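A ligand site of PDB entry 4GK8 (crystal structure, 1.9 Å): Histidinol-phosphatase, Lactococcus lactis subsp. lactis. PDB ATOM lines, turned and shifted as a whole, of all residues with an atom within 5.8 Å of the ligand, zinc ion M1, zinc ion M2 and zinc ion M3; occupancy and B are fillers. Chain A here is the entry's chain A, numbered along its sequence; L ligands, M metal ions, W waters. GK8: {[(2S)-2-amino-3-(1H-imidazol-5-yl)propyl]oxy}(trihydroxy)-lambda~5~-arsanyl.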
ATOM      1  N   HIS A   9     -16.186   5.190 -12.807  1.00  0.00           N
ATOM      2  CA  HIS A   9     -16.232   3.736 -12.667  1.00  0.00           C
ATOM      3  C   HIS A   9     -16.803   3.380 -11.297  1.00  0.00           C
ATOM      4  O   HIS A   9     -16.130   3.537 -10.289  1.00  0.00           O
ATOM      5  CB  HIS A   9     -14.830   3.120 -12.828  1.00  0.00           C
ATOM      6  CG  HIS A   9     -14.818   1.622 -12.918  1.00  0.00           C
ATOM      7  ND1 HIS A   9     -13.804   0.925 -13.534  1.00  0.00           N
ATOM      8  CD2 HIS A   9     -15.711   0.687 -12.489  1.00  0.00           C
ATOM      9  CE1 HIS A   9     -14.062  -0.375 -13.459  1.00  0.00           C
ATOM     10  NE2 HIS A   9     -15.214  -0.542 -12.838  1.00  0.00           N
ATOM     11  N   PHE A  10     -18.048   2.910 -11.277  1.00  0.00           N
ATOM     12  CA  PHE A  10     -18.658   2.455 -10.021  1.00  0.00           C
ATOM     13  C   PHE A  10     -19.929   1.670 -10.302  1.00  0.00           C
ATOM     14  O   PHE A  10     -20.470   1.699 -11.420  1.00  0.00           O
ATOM     15  CB  PHE A  10     -18.891   3.624  -9.028  1.00  0.00           C
ATOM     16  CG  PHE A  10     -19.811   4.702  -9.548  1.00  0.00           C
ATOM     17  CD1 PHE A  10     -21.179   4.649  -9.293  1.00  0.00           C
ATOM     18  CD2 PHE A  10     -19.304   5.783 -10.253  1.00  0.00           C
ATOM     19  CE1 PHE A  10     -22.030   5.636  -9.762  1.00  0.00           C
ATOM     20  CE2 PHE A  10     -20.140   6.768 -10.724  1.00  0.00           C
ATOM     21  CZ  PHE A  10     -21.514   6.698 -10.480  1.00  0.00           C
ATOM     22  N   HIS A  11     -20.400   0.944  -9.287  1.00  0.00           N
ATOM     23  CA  HIS A  11     -21.439  -0.064  -9.463  1.00  0.00           C
ATOM     24  C   HIS A  11     -22.547   0.058  -8.432  1.00  0.00           C
ATOM     25  O   HIS A  11     -22.280   0.391  -7.270  1.00  0.00           O
ATOM     26  CB  HIS A  11     -20.812  -1.446  -9.325  1.00  0.00           C
ATOM     27  CG  HIS A  11     -19.711  -1.706 -10.309  1.00  0.00           C
ATOM     28  ND1 HIS A  11     -19.934  -2.314 -11.522  1.00  0.00           N
ATOM     29  CD2 HIS A  11     -18.389  -1.435 -10.264  1.00  0.00           C
ATOM     30  CE1 HIS A  11     -18.802  -2.420 -12.183  1.00  0.00           C
ATOM     31  NE2 HIS A  11     -17.842  -1.888 -11.444  1.00  0.00           N
ATOM     32  N   SER A  15     -25.622  -4.115 -10.942  1.00  0.00           N
ATOM     33  CA  SER A  15     -24.509  -5.040 -11.168  1.00  0.00           C
ATOM     34  C   SER A  15     -24.655  -6.266 -10.294  1.00  0.00           C
ATOM     35  O   SER A  15     -25.129  -6.161  -9.161  1.00  0.00           O
ATOM     36  CB  SER A  15     -23.167  -4.374 -10.830  1.00  0.00           C
ATOM     37  OG  SER A  15     -22.823  -3.372 -11.775  1.00  0.00           O
ATOM     38  N   ASP A  17     -22.587  -7.971  -8.588  1.00  0.00           N
ATOM     39  CA  ASP A  17     -21.781  -8.057  -7.377  1.00  0.00           C
ATOM     40  C   ASP A  17     -21.867  -6.791  -6.511  1.00  0.00           C
ATOM     41  O   ASP A  17     -20.969  -6.519  -5.718  1.00  0.00           O
ATOM     42  CB  ASP A  17     -20.318  -8.366  -7.704  1.00  0.00           C
ATOM     43  CG  ASP A  17     -19.636  -7.263  -8.491  1.00  0.00           C
ATOM     44  OD1 ASP A  17     -20.341  -6.368  -8.980  1.00  0.00           O
ATOM     45  OD2 ASP A  17     -18.373  -7.298  -8.649  1.00  0.00           O
ATOM     46  N   THR A  40     -21.235   2.610 -14.195  1.00  0.00           N
ATOM     47  CA  THR A  40     -20.637   1.678 -15.144  1.00  0.00           C
ATOM     48  C   THR A  40     -20.918   0.245 -14.710  1.00  0.00           C
ATOM     49  O   THR A  40     -20.027  -0.454 -14.234  1.00  0.00           O
ATOM     50  CB  THR A  40     -19.099   1.875 -15.302  1.00  0.00           C
ATOM     51  OG1 THR A  40     -18.455   1.713 -14.044  1.00  0.00           O
ATOM     52  CG2 THR A  40     -18.758   3.271 -15.862  1.00  0.00           C
ATOM     53  N   HIS A  42     -21.859  -3.813 -14.516  1.00  0.00           N
ATOM     54  CA  HIS A  42     -21.277  -5.009 -15.155  1.00  0.00           C
ATOM     55  C   HIS A  42     -22.150  -5.664 -16.208  1.00  0.00           C
ATOM     56  O   HIS A  42     -23.335  -5.962 -15.946  1.00  0.00           O
ATOM     57  CB  HIS A  42     -21.051  -6.102 -14.095  1.00  0.00           C
ATOM     58  CG  HIS A  42     -19.857  -5.883 -13.208  1.00  0.00           C
ATOM     59  ND1 HIS A  42     -18.573  -5.771 -13.708  1.00  0.00           N
ATOM     60  CD2 HIS A  42     -19.752  -5.822 -11.864  1.00  0.00           C
ATOM     61  CE1 HIS A  42     -17.735  -5.626 -12.702  1.00  0.00           C
ATOM     62  NE2 HIS A  42     -18.422  -5.658 -11.577  1.00  0.00           N
ATOM     63  N   ASP A  44     -20.863  -9.236 -18.290  1.00  0.00           N
ATOM     64  CA  ASP A  44     -19.850 -10.212 -18.714  1.00  0.00           C
ATOM     65  C   ASP A  44     -20.617 -11.429 -19.256  1.00  0.00           C
ATOM     66  O   ASP A  44     -21.469 -11.961 -18.554  1.00  0.00           O
ATOM     67  CB  ASP A  44     -18.998 -10.692 -17.520  1.00  0.00           C
ATOM     68  CG  ASP A  44     -18.156  -9.571 -16.882  1.00  0.00           C
ATOM     69  OD1 ASP A  44     -18.726  -8.753 -16.115  1.00  0.00           O
ATOM     70  OD2 ASP A  44     -16.925  -9.533 -17.101  1.00  0.00           O
ATOM     71  N   PHE A  47     -20.081 -15.836 -17.880  1.00  0.00           N
ATOM     72  CA  PHE A  47     -19.041 -15.706 -16.872  1.00  0.00           C
ATOM     73  C   PHE A  47     -18.956 -16.961 -16.029  1.00  0.00           C
ATOM     74  O   PHE A  47     -19.985 -17.536 -15.695  1.00  0.00           O
ATOM     75  CB  PHE A  47     -19.271 -14.497 -15.963  1.00  0.00           C
ATOM     76  CG  PHE A  47     -18.029 -14.020 -15.257  1.00  0.00           C
ATOM     77  CD1 PHE A  47     -17.052 -13.334 -15.972  1.00  0.00           C
ATOM     78  CD2 PHE A  47     -17.813 -14.294 -13.919  1.00  0.00           C
ATOM     79  CE1 PHE A  47     -15.895 -12.891 -15.345  1.00  0.00           C
ATOM     80  CE2 PHE A  47     -16.656 -13.859 -13.280  1.00  0.00           C
ATOM     81  CZ  PHE A  47     -15.697 -13.157 -13.993  1.00  0.00           C
ATOM     82  N   MET A  50     -20.750 -17.347 -11.895  1.00  0.00           N
ATOM     83  CA  MET A  50     -21.678 -16.313 -11.469  1.00  0.00           C
ATOM     84  C   MET A  50     -22.139 -15.482 -12.658  1.00  0.00           C
ATOM     85  O   MET A  50     -21.329 -15.058 -13.478  1.00  0.00           O
ATOM     86  CB  MET A  50     -20.977 -15.409 -10.456  1.00  0.00           C
ATOM     87  CG  MET A  50     -21.792 -14.212  -9.996  1.00  0.00           C
ATOM     88  SD  MET A  50     -20.808 -13.271  -8.813  1.00  0.00           S
ATOM     89  CE  MET A  50     -21.910 -11.905  -8.499  1.00  0.00           C
ATOM     90  N   PHE A  52     -23.209 -12.363 -14.675  1.00  0.00           N
ATOM     91  CA  PHE A  52     -23.148 -10.906 -14.670  1.00  0.00           C
ATOM     92  C   PHE A  52     -24.042 -10.352 -15.767  1.00  0.00           C
ATOM     93  O   PHE A  52     -23.582  -9.928 -16.822  1.00  0.00           O
ATOM     94  CB  PHE A  52     -21.694 -10.409 -14.837  1.00  0.00           C
ATOM     95  CG  PHE A  52     -20.899 -10.455 -13.566  1.00  0.00           C
ATOM     96  CD1 PHE A  52     -20.841  -9.350 -12.729  1.00  0.00           C
ATOM     97  CD2 PHE A  52     -20.230 -11.604 -13.196  1.00  0.00           C
ATOM     98  CE1 PHE A  52     -20.111  -9.385 -11.560  1.00  0.00           C
ATOM     99  CE2 PHE A  52     -19.490 -11.636 -12.016  1.00  0.00           C
ATOM    100  CZ  PHE A  52     -19.435 -10.532 -11.197  1.00  0.00           C
ATOM    101  N   GLU A  81     -19.449  -1.306 -17.723  1.00  0.00           N
ATOM    102  CA  GLU A  81     -18.171  -2.003 -17.673  1.00  0.00           C
ATOM    103  C   GLU A  81     -18.349  -3.344 -18.347  1.00  0.00           C
ATOM    104  O   GLU A  81     -18.982  -4.248 -17.803  1.00  0.00           O
ATOM    105  CB  GLU A  81     -17.628  -2.180 -16.245  1.00  0.00           C
ATOM    106  CG  GLU A  81     -16.227  -2.828 -16.275  1.00  0.00           C
ATOM    107  CD  GLU A  81     -15.684  -3.233 -14.910  1.00  0.00           C
ATOM    108  OE1 GLU A  81     -16.386  -3.119 -13.892  1.00  0.00           O
ATOM    109  OE2 GLU A  81     -14.509  -3.681 -14.876  1.00  0.00           O
ATOM    110  N   SER A 107     -12.776  -4.382 -20.027  1.00  0.00           N
ATOM    111  CA  SER A 107     -12.029  -4.977 -18.928  1.00  0.00           C
ATOM    112  C   SER A 107     -11.794  -6.450 -19.209  1.00  0.00           C
ATOM    113  O   SER A 107     -12.599  -7.096 -19.880  1.00  0.00           O
ATOM    114  CB  SER A 107     -12.839  -4.880 -17.635  1.00  0.00           C
ATOM    115  OG  SER A 107     -12.912  -3.544 -17.160  1.00  0.00           O
ATOM    116  N   HIS A 109     -11.661  -9.879 -17.110  1.00  0.00           N
ATOM    117  CA  HIS A 109     -12.043 -10.453 -15.817  1.00  0.00           C
ATOM    118  C   HIS A 109     -11.867 -11.967 -15.770  1.00  0.00           C
ATOM    119  O   HIS A 109     -11.824 -12.584 -14.696  1.00  0.00           O
ATOM    120  CB  HIS A 109     -13.503 -10.129 -15.496  1.00  0.00           C
ATOM    121  CG  HIS A 109     -13.763  -8.678 -15.246  1.00  0.00           C
ATOM    122  ND1 HIS A 109     -14.884  -8.032 -15.718  1.00  0.00           N
ATOM    123  CD2 HIS A 109     -13.049  -7.741 -14.564  1.00  0.00           C
ATOM    124  CE1 HIS A 109     -14.849  -6.762 -15.346  1.00  0.00           C
ATOM    125  NE2 HIS A 109     -13.753  -6.556 -14.642  1.00  0.00           N
ATOM    126  N   GLU A 115     -11.777 -17.526 -13.995  1.00  0.00           N
ATOM    127  CA  GLU A 115     -11.867 -16.174 -13.459  1.00  0.00           C
ATOM    128  C   GLU A 115     -10.562 -15.712 -12.798  1.00  0.00           C
ATOM    129  O   GLU A 115      -9.919 -16.460 -12.064  1.00  0.00           O
ATOM    130  CB  GLU A 115     -13.024 -16.060 -12.450  1.00  0.00           C
ATOM    131  CG  GLU A 115     -13.132 -14.670 -11.848  1.00  0.00           C
ATOM    132  CD  GLU A 115     -14.240 -14.548 -10.817  1.00  0.00           C
ATOM    133  OE1 GLU A 115     -14.761 -15.577 -10.363  1.00  0.00           O
ATOM    134  OE2 GLU A 115     -14.579 -13.401 -10.473  1.00  0.00           O
ATOM    135  N   VAL A 116     -10.163 -14.481 -13.087  1.00  0.00           N
ATOM    136  CA  VAL A 116      -9.027 -13.867 -12.410  1.00  0.00           C
ATOM    137  C   VAL A 116      -9.555 -13.284 -11.097  1.00  0.00           C
ATOM    138  O   VAL A 116     -10.168 -12.220 -11.086  1.00  0.00           O
ATOM    139  CB  VAL A 116      -8.382 -12.767 -13.290  1.00  0.00           C
ATOM    140  CG1 VAL A 116      -7.150 -12.159 -12.593  1.00  0.00           C
ATOM    141  CG2 VAL A 116      -8.015 -13.342 -14.653  1.00  0.00           C
ATOM    142  N   TYR A 117      -9.342 -13.987  -9.990  1.00  0.00           N
ATOM    143  CA  TYR A 117      -9.946 -13.592  -8.728  1.00  0.00           C
ATOM    144  C   TYR A 117      -9.353 -14.409  -7.609  1.00  0.00           C
ATOM    145  O   TYR A 117      -8.672 -15.386  -7.867  1.00  0.00           O
ATOM    146  CB  TYR A 117     -11.465 -13.793  -8.767  1.00  0.00           C
ATOM    147  CG  TYR A 117     -12.206 -12.917  -7.774  1.00  0.00           C
ATOM    148  CD1 TYR A 117     -12.338 -11.549  -7.999  1.00  0.00           C
ATOM    149  CD2 TYR A 117     -12.787 -13.458  -6.631  1.00  0.00           C
ATOM    150  CE1 TYR A 117     -13.012 -10.731  -7.104  1.00  0.00           C
ATOM    151  CE2 TYR A 117     -13.467 -12.642  -5.729  1.00  0.00           C
ATOM    152  CZ  TYR A 117     -13.568 -11.285  -5.970  1.00  0.00           C
ATOM    153  OH  TYR A 117     -14.245 -10.468  -5.092  1.00  0.00           O
ATOM    154  N   HIS A 154      -8.762  -0.938 -15.427  1.00  0.00           N
ATOM    155  CA  HIS A 154      -7.810  -1.500 -14.462  1.00  0.00           C
ATOM    156  C   HIS A 154      -6.728  -2.459 -14.986  1.00  0.00           C
ATOM    157  O   HIS A 154      -6.849  -3.670 -14.866  1.00  0.00           O
ATOM    158  CB  HIS A 154      -8.567  -2.151 -13.269  1.00  0.00           C
ATOM    159  CG  HIS A 154      -9.664  -3.100 -13.666  1.00  0.00           C
ATOM    160  ND1 HIS A 154      -9.503  -4.094 -14.612  1.00  0.00           N
ATOM    161  CD2 HIS A 154     -10.936  -3.215 -13.226  1.00  0.00           C
ATOM    162  CE1 HIS A 154     -10.632  -4.784 -14.726  1.00  0.00           C
ATOM    163  NE2 HIS A 154     -11.521  -4.273 -13.896  1.00  0.00           N
ATOM    164  N   TYR A 157      -5.501  -5.000 -12.470  1.00  0.00           N
ATOM    165  CA  TYR A 157      -6.518  -5.896 -11.905  1.00  0.00           C
ATOM    166  C   TYR A 157      -5.915  -7.176 -11.315  1.00  0.00           C
ATOM    167  O   TYR A 157      -6.303  -7.630 -10.230  1.00  0.00           O
ATOM    168  CB  TYR A 157      -7.555  -6.239 -12.982  1.00  0.00           C
ATOM    169  CG  TYR A 157      -8.778  -7.022 -12.534  1.00  0.00           C
ATOM    170  CD1 TYR A 157      -9.847  -6.388 -11.907  1.00  0.00           C
ATOM    171  CD2 TYR A 157      -8.892  -8.387 -12.814  1.00  0.00           C
ATOM    172  CE1 TYR A 157     -10.979  -7.103 -11.534  1.00  0.00           C
ATOM    173  CE2 TYR A 157     -10.017  -9.107 -12.436  1.00  0.00           C
ATOM    174  CZ  TYR A 157     -11.051  -8.455 -11.798  1.00  0.00           C
ATOM    175  OH  TYR A 157     -12.167  -9.164 -11.422  1.00  0.00           O
ATOM    176  N   ARG A 160      -4.738  -7.312  -7.704  1.00  0.00           N
ATOM    177  CA  ARG A 160      -5.666  -7.266  -6.583  1.00  0.00           C
ATOM    178  C   ARG A 160      -5.719  -8.601  -5.855  1.00  0.00           C
ATOM    179  O   ARG A 160      -6.042  -8.648  -4.671  1.00  0.00           O
ATOM    180  CB  ARG A 160      -7.072  -6.909  -7.039  1.00  0.00           C
ATOM    181  CG  ARG A 160      -7.203  -5.547  -7.720  1.00  0.00           C
ATOM    182  CD  ARG A 160      -8.605  -5.446  -8.314  1.00  0.00           C
ATOM    183  NE  ARG A 160      -8.884  -4.120  -8.865  1.00  0.00           N
ATOM    184  CZ  ARG A 160     -10.104  -3.740  -9.235  1.00  0.00           C
ATOM    185  NH1 ARG A 160     -11.111  -4.595  -9.088  1.00  0.00           N
ATOM    186  NH2 ARG A 160     -10.307  -2.517  -9.718  1.00  0.00           N
ATOM    187  N   TYR A 161      -5.438  -9.686  -6.560  1.00  0.00           N
ATOM    188  CA  TYR A 161      -5.832 -11.009  -6.069  1.00  0.00           C
ATOM    189  C   TYR A 161      -4.682 -11.992  -6.124  1.00  0.00           C
ATOM    190  O   TYR A 161      -3.631 -11.703  -6.673  1.00  0.00           O
ATOM    191  CB  TYR A 161      -7.019 -11.563  -6.876  1.00  0.00           C
ATOM    192  CG  TYR A 161      -8.111 -10.547  -7.154  1.00  0.00           C
ATOM    193  CD1 TYR A 161      -8.949 -10.113  -6.131  1.00  0.00           C
ATOM    194  CD2 TYR A 161      -8.295 -10.024  -8.435  1.00  0.00           C
ATOM    195  CE1 TYR A 161      -9.957  -9.166  -6.380  1.00  0.00           C
ATOM    196  CE2 TYR A 161      -9.289  -9.081  -8.686  1.00  0.00           C
ATOM    197  CZ  TYR A 161     -10.115  -8.665  -7.659  1.00  0.00           C
ATOM    198  OH  TYR A 161     -11.102  -7.727  -7.905  1.00  0.00           O
ATOM    199  N   ASN A 195      -7.518   3.600 -12.169  1.00  0.00           N
ATOM    200  CA  ASN A 195      -8.453   2.940 -11.262  1.00  0.00           C
ATOM    201  C   ASN A 195      -7.907   3.026  -9.844  1.00  0.00           C
ATOM    202  O   ASN A 195      -6.801   2.565  -9.581  1.00  0.00           O
ATOM    203  CB  ASN A 195      -8.621   1.471 -11.699  1.00  0.00           C
ATOM    204  CG  ASN A 195      -9.745   0.767 -10.959  1.00  0.00           C
ATOM    205  OD1 ASN A 195      -9.768   0.721  -9.730  1.00  0.00           O
ATOM    206  ND2 ASN A 195     -10.682   0.213 -11.712  1.00  0.00           N
ATOM    207  N   ARG A 197      -8.797   1.642  -6.959  1.00  0.00           N
ATOM    208  CA  ARG A 197      -9.071   0.559  -6.016  1.00  0.00           C
ATOM    209  C   ARG A 197      -7.910   0.282  -5.043  1.00  0.00           C
ATOM    210  O   ARG A 197      -8.122   0.256  -3.831  1.00  0.00           O
ATOM    211  CB  ARG A 197      -9.479  -0.730  -6.736  1.00  0.00           C
ATOM    212  CG  ARG A 197      -9.574  -1.949  -5.783  1.00  0.00           C
ATOM    213  CD  ARG A 197     -10.763  -1.882  -4.819  1.00  0.00           C
ATOM    214  NE  ARG A 197     -12.039  -1.886  -5.542  1.00  0.00           N
ATOM    215  CZ  ARG A 197     -12.588  -2.972  -6.088  1.00  0.00           C
ATOM    216  NH1 ARG A 197     -11.990  -4.147  -5.993  1.00  0.00           N
ATOM    217  NH2 ARG A 197     -13.737  -2.868  -6.753  1.00  0.00           N
ATOM    218  N   ASP A 228     -14.045   2.460  -8.812  1.00  0.00           N
ATOM    219  CA  ASP A 228     -14.507   1.072  -8.806  1.00  0.00           C
ATOM    220  C   ASP A 228     -15.304   0.726  -7.535  1.00  0.00           C
ATOM    221  O   ASP A 228     -15.326  -0.421  -7.099  1.00  0.00           O
ATOM    222  CB  ASP A 228     -13.347   0.087  -8.979  1.00  0.00           C
ATOM    223  CG  ASP A 228     -13.708  -1.094  -9.874  1.00  0.00           C
ATOM    224  OD1 ASP A 228     -14.910  -1.381 -10.067  1.00  0.00           O
ATOM    225  OD2 ASP A 228     -12.775  -1.730 -10.391  1.00  0.00           O
ATOM    226  N   HIS A 230     -18.213  -0.293  -5.106  1.00  0.00           N
ATOM    227  CA  HIS A 230     -19.430  -1.079  -5.179  1.00  0.00           C
ATOM    228  C   HIS A 230     -20.380  -0.661  -4.055  1.00  0.00           C
ATOM    229  O   HIS A 230     -21.494  -1.156  -3.962  1.00  0.00           O
ATOM    230  CB  HIS A 230     -19.123  -2.572  -5.113  1.00  0.00           C
ATOM    231  CG  HIS A 230     -18.436  -3.082  -6.349  1.00  0.00           C
ATOM    232  ND1 HIS A 230     -17.275  -2.527  -6.832  1.00  0.00           N
ATOM    233  CD2 HIS A 230     -18.759  -4.088  -7.192  1.00  0.00           C
ATOM    234  CE1 HIS A 230     -16.910  -3.175  -7.923  1.00  0.00           C
ATOM    235  NE2 HIS A 230     -17.793  -4.131  -8.162  1.00  0.00           N
HETATM  236  C   GK8 L   1     -15.119  -7.717  -9.762  1.00  0.00           C
HETATM  237  N   GK8 L   1     -15.312  -8.557 -12.019  1.00  0.00           N
HETATM  238 AS   GK8 L   1     -14.783  -5.105 -10.562  1.00  0.00          AS
HETATM  239  O1  GK8 L   1     -13.527  -4.692  -9.394  1.00  0.00           O
HETATM  240  O2  GK8 L   1     -14.185  -5.877 -12.055  1.00  0.00           O
HETATM  241  O3  GK8 L   1     -16.015  -3.881 -10.889  1.00  0.00           O
HETATM  242  O4  GK8 L   1     -15.665  -6.446  -9.746  1.00  0.00           O
HETATM  243  CA  GK8 L   1     -15.742  -8.754 -10.660  1.00  0.00           C
HETATM  244  CB  GK8 L   1     -15.386 -10.149 -10.231  1.00  0.00           C
HETATM  245  CG  GK8 L   1     -16.183 -10.804  -9.148  1.00  0.00           C
HETATM  246  ND1 GK8 L   1     -16.282 -12.137  -8.905  1.00  0.00           N
HETATM  247  CD2 GK8 L   1     -16.975 -10.175  -8.186  1.00  0.00           C
HETATM  248  CE1 GK8 L   1     -17.081 -12.331  -7.855  1.00  0.00           C
HETATM  249  NE2 GK8 L   1     -17.500 -11.144  -7.418  1.00  0.00           N
HETATM  250 ZN    ZN M   1     -13.553  -4.807 -13.541  1.00  0.00          ZN
HETATM  251 ZN    ZN M   2     -17.651  -5.612  -9.644  1.00  0.00          ZN
HETATM  252 ZN    ZN M   3     -15.784  -2.364 -11.898  1.00  0.00          ZN
HETATM  253  O   HOH W   1     -17.269  -9.193 -13.575  1.00  0.00           O
HETATM  254  O   HOH W   2     -13.904  -3.235 -12.256  1.00  0.00           O
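O2 of the ligand binds zinc ion M1 (1.9 Å).
The side-chain carboxylate (OE2) of Glu 81 is bound to zinc ion M1 (2.0 Å).
Zinc ion M1 is bound by water W2 (2.1 Å).
A ring nitrogen (NE2) of His 109 is bound to zinc ion M1 (2.1 Å).
NE2 of His 154 binds zinc ion M1 (2.1 Å).
The side-chain carboxylate (OE1) of Glu 81 lies close to a ring nitrogen (ND1) of His 42 (3.4 Å).
OD2 of Asp 44 sits at hydrogen-bond distance from ND1 of His 109.
N of His 42 lies within hydrogen-bond range of OG of Ser 15 (2.9 Å).
The backbone carbonyl oxygen of Thr 40 lies close to a ring nitrogen (ND1) of His 11 (3.3 Å).
OG of Ser 15 is in hydrogen-bond range of ND1 of His 11 (3.1 Å).
The guanidinium group of Arg 160 sits at hydrogen-bond distance from the side-chain hydroxyl of Tyr 161 (3.3 Å).
The backbone NH of Arg 197 lies within hydrogen-bond range of the side-chain amide oxygen of Asn 195 (3.1 Å).
The backbone carbonyl oxygen of Phe 52 sits at hydrogen-bond distance from the backbone NH of Asp 44, 3.2 Å away.
Zinc ion M2 is bound by a ring nitrogen (NE2) of His 42, the side-chain carboxylate (OD2) of Asp 17, a ring nitrogen (NE2) of His 230 and an oxygen (O4) of the ligand.
Zinc ion M2 has four donor atoms within binding distance.
Slightly farther from zinc ion M2 lies an oxygen (O3) of the ligand (2.7 Å).
An oxygen (O1) of the ligand sits at hydrogen-bond distance from the guanidinium group (NH1) of Arg 160 (2.4 Å).
The side-chain carboxylate (OE2) of Glu 115 sits at hydrogen-bond distance from a nitrogen (ND1) of the ligand (2.6 Å).
An oxygen (O1) of the ligand sits at hydrogen-bond distance from the guanidinium group (NH2) of Arg 197 (3.2 Å).
The side-chain hydroxyl (OH) of Tyr 157 lies within hydrogen-bond range of a nitrogen (N) of the ligand (3.3 Å).
Merely in contact with the ligand: Met 50 (3.96 Å), Phe 52 (3.9 Å) and Tyr 117 (3.8 Å).
Hydrophobic or aromatic side chains that line the ligand: His 11, His 42, Met 50, Phe 52, His 109, Tyr 117, Tyr 157 and His 230.
Of the 25 residues printed, 16 come within 4 Å of the ligand.
Three residues have an atom within 4 Å of zinc ion M2: Asp 17, His 42 and His 230.
Within 4 Å of zinc ion M3: His 9, His 11, His 42, Glu 81 and Asp 228.
The nearest printed residue that does not touch zinc ion M3 is His 230 (4.2 Å).
Water W2 lies within hydrogen-bond range of OD2 of Asp 228 (2.6 Å) and O1 of the ligand (3.2 Å).
Water W1 lies within hydrogen-bond range of a nitrogen (N) of the ligand (2.6 Å), the side-chain carboxylate of Asp 44 (3.0 Å) and a ring nitrogen (ND1) of His 109 (3.4 Å).
O3 of the ligand binds zinc ion M3, 1.8 Å away.
Water W2 binds zinc ion M3.
Zinc ion M3 is bound by a ring nitrogen (NE2) of His 9 (2.1 Å).
A ring nitrogen (NE2) of His 11 is bound to zinc ion M3.
Zinc ion M3 is bound by the side-chain carboxylate (OE1) of Glu 81, 2.2 Å away.
OD1 of Asp 228 binds zinc ion M3 (2.3 Å).
Zinc ion M3 has six donor atoms within binding distance.
OG of Ser 107 touches zinc ion M1, at 3.9 Å.
Tyr 157 touches zinc ion M1.
Of the 25 residues printed, 5 come within 4 Å of zinc ion M1.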
